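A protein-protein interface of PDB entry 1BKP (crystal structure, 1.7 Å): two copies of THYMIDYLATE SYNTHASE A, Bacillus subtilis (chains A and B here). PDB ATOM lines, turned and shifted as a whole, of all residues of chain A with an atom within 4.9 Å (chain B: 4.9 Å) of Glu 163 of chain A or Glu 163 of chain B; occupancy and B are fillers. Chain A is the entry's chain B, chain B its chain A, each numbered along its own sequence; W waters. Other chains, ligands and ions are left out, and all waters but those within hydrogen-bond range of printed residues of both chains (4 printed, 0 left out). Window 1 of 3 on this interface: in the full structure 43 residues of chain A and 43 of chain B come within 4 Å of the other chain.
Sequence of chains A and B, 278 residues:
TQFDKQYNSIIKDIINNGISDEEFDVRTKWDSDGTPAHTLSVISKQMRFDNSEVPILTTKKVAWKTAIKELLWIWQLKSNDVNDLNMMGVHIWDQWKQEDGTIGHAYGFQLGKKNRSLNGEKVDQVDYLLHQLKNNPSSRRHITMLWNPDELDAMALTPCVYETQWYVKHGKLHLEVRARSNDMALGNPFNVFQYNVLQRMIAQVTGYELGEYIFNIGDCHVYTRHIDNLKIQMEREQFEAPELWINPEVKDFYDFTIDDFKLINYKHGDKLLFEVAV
OE1 of Glu 163 of chain A lies within hydrogen-bond range of OH of Tyr 162 of chain B. OH of Tyr 162 of chain A sits at hydrogen-bond distance from OE1 of Glu 163 of chain B, at 2.6 Å. OE2 of Glu 163 of chain B lies close to OE2 of Glu 163 of chain A, 2.6 Å away. The guanidinium group of Arg 178 of chain A is in hydrogen-bond range of the side-chain amide oxygen of Gln 165 of chain B (2.8 Å). The side-chain carboxylate (OE1) of Glu 176 of chain B lies within salt-bridge range of the guanidinium group (NH2) of Arg 178 of chain A. NH1 of Arg 178 of chain B sits at hydrogen-bond distance from OE1 of Gln 165 of chain A, 2.8 Å away. The side-chain carboxylate (OE1) of Glu 176 of chain A is in salt-bridge range of the guanidinium group (NH2) of Arg 178 of chain B (2.9 Å).
Of the 10 printed residues of chain B, 6 touch a printed residue of chain A. Among the printed residues, 9 pairs touch across the chains. Among the printed residues, Asp or Glu carboxylates within 4 Å of a Lys or Arg side-chain nitrogen of the other chain: Glu 176 of chain A with Arg 178 of chain B (2.9 Å) and Arg 178 of chain A with Glu 176 of chain B (3.0 Å).
Water W3 lies within hydrogen-bond range of the side-chain carboxylate of Glu 176 of chain A (2.7 Å) and the guanidinium group of Arg 178 of chain B (2.8 Å). Water W4 lies within hydrogen-bond range of OE2 of Glu 176 of chain B and NE of Arg 178 of chain A. Water W1 lies within hydrogen-bond range of OE1 of Glu 163 of chain A (3.0 Å), O of Thr 164 of chain A (3.0 Å), OH of Tyr 162 of chain B (3.2 Å) and NH1 of Arg 178 of chain B (3.4 Å). Water W2 lies within hydrogen-bond range of the backbone carbonyl oxygen (O) of Thr 164 of chain B (3.0 Å), the side-chain carboxylate (OE1) of Glu 163 of chain B (3.1 Å), the side-chain hydroxyl (OH) of Tyr 162 of chain A (3.2 Å) and the guanidinium group (NH1) of Arg 178 of chain A (3.4 Å).
The side-chain carboxylate (OE2) of Glu 163 of chain B is in hydrogen-bond range of the side-chain hydroxyl (OH) of Tyr 162 of chain B (3.1 Å). The guanidinium group (NH1) of Arg 178 of chain B lies within hydrogen-bond range of the side-chain hydroxyl (OH) of Tyr 162 of chain B (2.8 Å). The backbone carbonyl oxygen (O) of Glu 176 of chain B lies within hydrogen-bond range of the backbone NH (N) of Gln 165 of chain B (2.8 Å). OH of Tyr 162 of chain A sits at hydrogen-bond distance from OE2 of Glu 163 of chain A. The backbone carbonyl oxygen of Glu 163 of chain A is in hydrogen-bond range of the backbone NH of Arg 178 of chain A, at 3.2 Å. N of Gln 165 of chain A sits at hydrogen-bond distance from O of Glu 176 of chain A, at 2.9 Å.
Met 145 of chain B touches Met 145 of chain A. Met 145 of chain A touches Tyr 162 of chain B (CE to CE2, 3.95 Å).
Of the printed residues of chain B, Glu 163 of chain A touches Tyr 162 (2.7 Å) and Glu 163 (2.6 Å). Glu 163 of chain B touches just these residues of chain A: Tyr 162 (2.6 Å) and Glu 163 (2.6 Å). Printed residues of chain B within 4 Å of Glu 176 of chain A: Arg 178. Of the printed residues of chain A, Tyr 162 of chain B touches Met 145 (3.95 Å) and Glu 163 (2.7 Å).
Met 145 of chain A touches Tyr 162 of chain B, but with the chains exchanged Tyr 162 of chain A does not touch Met 145 of chain B (4.1 Å). Tyr 162 of chain A touches Glu 163 of chain B, and with the chains exchanged Glu 163 of chain A touches Tyr 162 of chain B. Glu 163 of chain A touches its own counterpart, Glu 163 of chain B. Gln 165 of chain A touches Arg 178 of chain B, and with the chains exchanged Arg 178 of chain A touches Gln 165 of chain B. Positions printed for both chains: 144, 145, 161, 162, 163, 164, 165, 176, 177 and 178.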
ATOM      1  N   THR A 144       3.910  13.163  21.528  1.00  0.00           N
ATOM      2  CA  THR A 144       2.861  12.397  20.885  1.00  0.00           C
ATOM      3  C   THR A 144       3.545  11.959  19.572  1.00  0.00           C
ATOM      4  O   THR A 144       4.433  12.680  19.044  1.00  0.00           O
ATOM      5  CB  THR A 144       1.552  13.226  20.554  1.00  0.00           C
ATOM      6  OG1 THR A 144       1.882  14.338  19.668  1.00  0.00           O
ATOM      7  CG2 THR A 144       0.955  13.728  21.819  1.00  0.00           C
ATOM      8  N   MET A 145       3.120  10.846  19.016  1.00  0.00           N
ATOM      9  CA  MET A 145       3.788  10.269  17.838  1.00  0.00           C
ATOM     10  C   MET A 145       2.752   9.677  16.926  1.00  0.00           C
ATOM     11  O   MET A 145       2.013   8.751  17.373  1.00  0.00           O
ATOM     12  CB  MET A 145       4.710   9.101  18.367  1.00  0.00           C
ATOM     13  CG  MET A 145       5.604   8.363  17.287  1.00  0.00           C
ATOM     14  SD  MET A 145       6.531   9.501  16.353  1.00  0.00           S
ATOM     15  CE  MET A 145       7.671  10.320  17.564  1.00  0.00           C
ATOM     16  N   VAL A 161       3.312  16.112   9.554  1.00  0.00           N
ATOM     17  CA  VAL A 161       3.598  16.709  10.909  1.00  0.00           C
ATOM     18  C   VAL A 161       3.263  15.480  11.794  1.00  0.00           C
ATOM     19  O   VAL A 161       2.072  15.192  12.061  1.00  0.00           O
ATOM     20  CB  VAL A 161       2.672  17.955  11.272  1.00  0.00           C
ATOM     21  CG1 VAL A 161       3.060  18.572  12.633  1.00  0.00           C
ATOM     22  CG2 VAL A 161       2.735  18.920  10.207  1.00  0.00           C
ATOM     23  N   TYR A 162       4.296  14.770  12.251  1.00  0.00           N
ATOM     24  CA  TYR A 162       3.999  13.490  12.882  1.00  0.00           C
ATOM     25  C   TYR A 162       4.325  13.448  14.368  1.00  0.00           C
ATOM     26  O   TYR A 162       4.096  12.416  14.983  1.00  0.00           O
ATOM     27  CB  TYR A 162       4.770  12.353  12.137  1.00  0.00           C
ATOM     28  CG  TYR A 162       6.290  12.488  12.272  1.00  0.00           C
ATOM     29  CD1 TYR A 162       7.041  13.357  11.452  1.00  0.00           C
ATOM     30  CD2 TYR A 162       6.976  11.841  13.329  1.00  0.00           C
ATOM     31  CE1 TYR A 162       8.416  13.555  11.666  1.00  0.00           C
ATOM     32  CE2 TYR A 162       8.358  12.082  13.567  1.00  0.00           C
ATOM     33  CZ  TYR A 162       9.068  12.942  12.694  1.00  0.00           C
ATOM     34  OH  TYR A 162      10.451  13.054  12.885  1.00  0.00           O
ATOM     35  N   GLU A 163       4.885  14.521  14.906  1.00  0.00           N
ATOM     36  CA  GLU A 163       5.193  14.493  16.316  1.00  0.00           C
ATOM     37  C   GLU A 163       5.195  15.802  17.025  1.00  0.00           C
ATOM     38  O   GLU A 163       5.468  16.893  16.439  1.00  0.00           O
ATOM     39  CB  GLU A 163       6.600  13.821  16.594  1.00  0.00           C
ATOM     40  CG  GLU A 163       7.790  14.654  15.979  1.00  0.00           C
ATOM     41  CD  GLU A 163       9.174  14.129  16.321  1.00  0.00           C
ATOM     42  OE1 GLU A 163       9.304  13.304  17.222  1.00  0.00           O
ATOM     43  OE2 GLU A 163      10.152  14.579  15.681  1.00  0.00           O
ATOM     44  N   THR A 164       4.976  15.725  18.349  1.00  0.00           N
ATOM     45  CA  THR A 164       5.095  16.967  19.148  1.00  0.00           C
ATOM     46  C   THR A 164       5.823  16.632  20.472  1.00  0.00           C
ATOM     47  O   THR A 164       5.915  15.504  20.852  1.00  0.00           O
ATOM     48  CB  THR A 164       3.683  17.528  19.557  1.00  0.00           C
ATOM     49  OG1 THR A 164       3.084  16.643  20.509  1.00  0.00           O
ATOM     50  CG2 THR A 164       2.698  17.600  18.295  1.00  0.00           C
ATOM     51  N   GLN A 165       6.444  17.597  21.057  1.00  0.00           N
ATOM     52  CA  GLN A 165       7.015  17.418  22.390  1.00  0.00           C
ATOM     53  C   GLN A 165       6.573  18.715  23.119  1.00  0.00           C
ATOM     54  O   GLN A 165       6.713  19.860  22.591  1.00  0.00           O
ATOM     55  CB  GLN A 165       8.526  17.320  22.374  1.00  0.00           C
ATOM     56  CG  GLN A 165       9.039  17.016  23.855  1.00  0.00           C
ATOM     57  CD  GLN A 165      10.494  16.588  23.877  1.00  0.00           C
ATOM     58  OE1 GLN A 165      11.120  16.417  22.868  1.00  0.00           O
ATOM     59  NE2 GLN A 165      11.008  16.354  25.084  1.00  0.00           N
ATOM     60  N   GLU A 176       6.949  22.102  20.718  1.00  0.00           N
ATOM     61  CA  GLU A 176       7.894  21.940  19.601  1.00  0.00           C
ATOM     62  C   GLU A 176       7.257  20.864  18.673  1.00  0.00           C
ATOM     63  O   GLU A 176       6.868  19.766  19.155  1.00  0.00           O
ATOM     64  CB  GLU A 176       9.278  21.489  20.135  1.00  0.00           C
ATOM     65  CG  GLU A 176      10.234  21.293  19.035  1.00  0.00           C
ATOM     66  CD  GLU A 176      11.694  21.154  19.492  1.00  0.00           C
ATOM     67  OE1 GLU A 176      11.897  20.801  20.659  1.00  0.00           O
ATOM     68  OE2 GLU A 176      12.617  21.503  18.707  1.00  0.00           O
ATOM     69  N   VAL A 177       7.188  21.132  17.365  1.00  0.00           N
ATOM     70  CA  VAL A 177       6.637  20.138  16.498  1.00  0.00           C
ATOM     71  C   VAL A 177       7.585  19.854  15.321  1.00  0.00           C
ATOM     72  O   VAL A 177       8.504  20.678  15.057  1.00  0.00           O
ATOM     73  CB  VAL A 177       5.171  20.481  15.976  1.00  0.00           C
ATOM     74  CG1 VAL A 177       4.404  21.371  16.961  1.00  0.00           C
ATOM     75  CG2 VAL A 177       5.175  21.049  14.732  1.00  0.00           C
ATOM     76  N   ARG A 178       7.382  18.701  14.670  1.00  0.00           N
ATOM     77  CA  ARG A 178       8.243  18.372  13.536  1.00  0.00           C
ATOM     78  C   ARG A 178       7.461  17.796  12.431  1.00  0.00           C
ATOM     79  O   ARG A 178       6.678  16.845  12.631  1.00  0.00           O
ATOM     80  CB  ARG A 178       9.369  17.402  13.894  1.00  0.00           C
ATOM     81  CG  ARG A 178      10.412  17.196  12.706  1.00  0.00           C
ATOM     82  CD  ARG A 178      11.696  16.613  13.268  1.00  0.00           C
ATOM     83  NE  ARG A 178      12.665  16.591  12.162  1.00  0.00           N
ATOM     84  CZ  ARG A 178      12.789  15.651  11.213  1.00  0.00           C
ATOM     85  NH1 ARG A 178      12.030  14.523  11.165  1.00  0.00           N
ATOM     86  NH2 ARG A 178      13.701  15.865  10.240  1.00  0.00           N
ATOM     87  N   THR B 144      13.767   6.273  11.164  1.00  0.00           N
ATOM     88  CA  THR B 144      13.680   5.111  12.032  1.00  0.00           C
ATOM     89  C   THR B 144      13.155   5.765  13.297  1.00  0.00           C
ATOM     90  O   THR B 144      13.460   6.968  13.538  1.00  0.00           O
ATOM     91  CB  THR B 144      15.012   4.445  12.349  1.00  0.00           C
ATOM     92  OG1 THR B 144      15.953   5.380  12.909  1.00  0.00           O
ATOM     93  CG2 THR B 144      15.607   3.891  11.076  1.00  0.00           C
ATOM     94  N   MET B 145      12.557   4.930  14.118  1.00  0.00           N
ATOM     95  CA  MET B 145      11.824   5.374  15.307  1.00  0.00           C
ATOM     96  C   MET B 145      11.868   4.368  16.375  1.00  0.00           C
ATOM     97  O   MET B 145      11.330   3.230  16.177  1.00  0.00           O
ATOM     98  CB  MET B 145      10.302   5.513  14.853  1.00  0.00           C
ATOM     99  CG  MET B 145       9.292   6.066  15.933  1.00  0.00           C
ATOM    100  SD  MET B 145       9.854   7.586  16.583  1.00  0.00           S
ATOM    101  CE  MET B 145       9.871   8.634  15.133  1.00  0.00           C
ATOM    102  N   VAL B 161      17.864   9.262  22.485  1.00  0.00           N
ATOM    103  CA  VAL B 161      18.080   9.556  21.041  1.00  0.00           C
ATOM    104  C   VAL B 161      17.171   8.522  20.371  1.00  0.00           C
ATOM    105  O   VAL B 161      17.526   7.345  20.217  1.00  0.00           O
ATOM    106  CB  VAL B 161      19.601   9.377  20.621  1.00  0.00           C
ATOM    107  CG1 VAL B 161      19.726   9.756  19.137  1.00  0.00           C
ATOM    108  CG2 VAL B 161      20.566  10.239  21.538  1.00  0.00           C
ATOM    109  N   TYR B 162      16.002   8.970  19.964  1.00  0.00           N
ATOM    110  CA  TYR B 162      14.987   8.022  19.575  1.00  0.00           C
ATOM    111  C   TYR B 162      14.612   7.997  18.084  1.00  0.00           C
ATOM    112  O   TYR B 162      13.813   7.122  17.674  1.00  0.00           O
ATOM    113  CB  TYR B 162      13.707   8.341  20.437  1.00  0.00           C
ATOM    114  CG  TYR B 162      12.939   9.665  20.119  1.00  0.00           C
ATOM    115  CD1 TYR B 162      13.358  10.899  20.691  1.00  0.00           C
ATOM    116  CD2 TYR B 162      11.954   9.707  19.105  1.00  0.00           C
ATOM    117  CE1 TYR B 162      12.844  12.093  20.267  1.00  0.00           C
ATOM    118  CE2 TYR B 162      11.418  10.921  18.674  1.00  0.00           C
ATOM    119  CZ  TYR B 162      11.879  12.124  19.283  1.00  0.00           C
ATOM    120  OH  TYR B 162      11.356  13.331  18.953  1.00  0.00           O
ATOM    121  N   GLU B 163      15.096   8.958  17.304  1.00  0.00           N
ATOM    122  CA  GLU B 163      14.724   8.929  15.872  1.00  0.00           C
ATOM    123  C   GLU B 163      15.777   9.451  14.989  1.00  0.00           C
ATOM    124  O   GLU B 163      16.702  10.223  15.424  1.00  0.00           O
ATOM    125  CB  GLU B 163      13.379   9.732  15.612  1.00  0.00           C
ATOM    126  CG  GLU B 163      13.626  11.226  15.855  1.00  0.00           C
ATOM    127  CD  GLU B 163      12.385  12.090  15.520  1.00  0.00           C
ATOM    128  OE1 GLU B 163      11.532  11.663  14.765  1.00  0.00           O
ATOM    129  OE2 GLU B 163      12.306  13.208  15.982  1.00  0.00           O
ATOM    130  N   THR B 164      15.732   9.010  13.717  1.00  0.00           N
ATOM    131  CA  THR B 164      16.689   9.531  12.727  1.00  0.00           C
ATOM    132  C   THR B 164      15.900   9.777  11.446  1.00  0.00           C
ATOM    133  O   THR B 164      14.861   9.174  11.229  1.00  0.00           O
ATOM    134  CB  THR B 164      17.805   8.540  12.332  1.00  0.00           C
ATOM    135  OG1 THR B 164      17.275   7.390  11.639  1.00  0.00           O
ATOM    136  CG2 THR B 164      18.539   7.957  13.551  1.00  0.00           C
ATOM    137  N   GLN B 165      16.372  10.700  10.625  1.00  0.00           N
ATOM    138  CA  GLN B 165      15.775  10.908   9.274  1.00  0.00           C
ATOM    139  C   GLN B 165      17.015  11.028   8.345  1.00  0.00           C
ATOM    140  O   GLN B 165      17.970  11.726   8.644  1.00  0.00           O
ATOM    141  CB  GLN B 165      14.876  12.165   9.193  1.00  0.00           C
ATOM    142  CG  GLN B 165      14.312  12.223   7.761  1.00  0.00           C
ATOM    143  CD  GLN B 165      13.135  13.184   7.651  1.00  0.00           C
ATOM    144  OE1 GLN B 165      12.736  13.779   8.578  1.00  0.00           O
ATOM    145  NE2 GLN B 165      12.551  13.281   6.437  1.00  0.00           N
ATOM    146  N   GLU B 176      19.919  13.276  10.050  1.00  0.00           N
ATOM    147  CA  GLU B 176      19.409  14.203  11.066  1.00  0.00           C
ATOM    148  C   GLU B 176      18.925  13.318  12.228  1.00  0.00           C
ATOM    149  O   GLU B 176      18.128  12.411  12.040  1.00  0.00           O
ATOM    150  CB  GLU B 176      18.246  15.051  10.496  1.00  0.00           C
ATOM    151  CG  GLU B 176      17.750  16.052  11.502  1.00  0.00           C
ATOM    152  CD  GLU B 176      16.973  17.231  10.912  1.00  0.00           C
ATOM    153  OE1 GLU B 176      16.449  17.093   9.793  1.00  0.00           O
ATOM    154  OE2 GLU B 176      16.886  18.275  11.579  1.00  0.00           O
ATOM    155  N   VAL B 177      19.315  13.633  13.456  1.00  0.00           N
ATOM    156  CA  VAL B 177      18.943  12.807  14.595  1.00  0.00           C
ATOM    157  C   VAL B 177      18.246  13.690  15.644  1.00  0.00           C
ATOM    158  O   VAL B 177      18.527  14.866  15.718  1.00  0.00           O
ATOM    159  CB  VAL B 177      20.325  12.283  15.206  1.00  0.00           C
ATOM    160  CG1 VAL B 177      20.195  11.579  16.462  1.00  0.00           C
ATOM    161  CG2 VAL B 177      21.033  11.386  14.191  1.00  0.00           C
ATOM    162  N   ARG B 178      17.408  13.117  16.495  1.00  0.00           N
ATOM    163  CA  ARG B 178      16.832  13.928  17.583  1.00  0.00           C
ATOM    164  C   ARG B 178      16.851  13.201  18.892  1.00  0.00           C
ATOM    165  O   ARG B 178      16.442  12.020  18.947  1.00  0.00           O
ATOM    166  CB  ARG B 178      15.375  14.369  17.343  1.00  0.00           C
ATOM    167  CG  ARG B 178      14.897  15.460  18.401  1.00  0.00           C
ATOM    168  CD  ARG B 178      13.595  16.090  17.941  1.00  0.00           C
ATOM    169  NE  ARG B 178      13.226  17.115  18.900  1.00  0.00           N
ATOM    170  CZ  ARG B 178      12.539  16.927  20.008  1.00  0.00           C
ATOM    171  NH1 ARG B 178      11.876  15.793  20.206  1.00  0.00           N
ATOM    172  NH2 ARG B 178      12.336  17.953  20.813  1.00  0.00           N
HETATM  173  O   HOH W   1       8.639  14.927  19.657  1.00  0.00           O
HETATM  174  O   HOH W   2      13.122  11.449  12.153  1.00  0.00           O
HETATM  175  O   HOH W   3      14.525  19.548  18.517  1.00  0.00           O
HETATM  176  O   HOH W   4      14.162  19.190  11.598  1.00  0.00           O
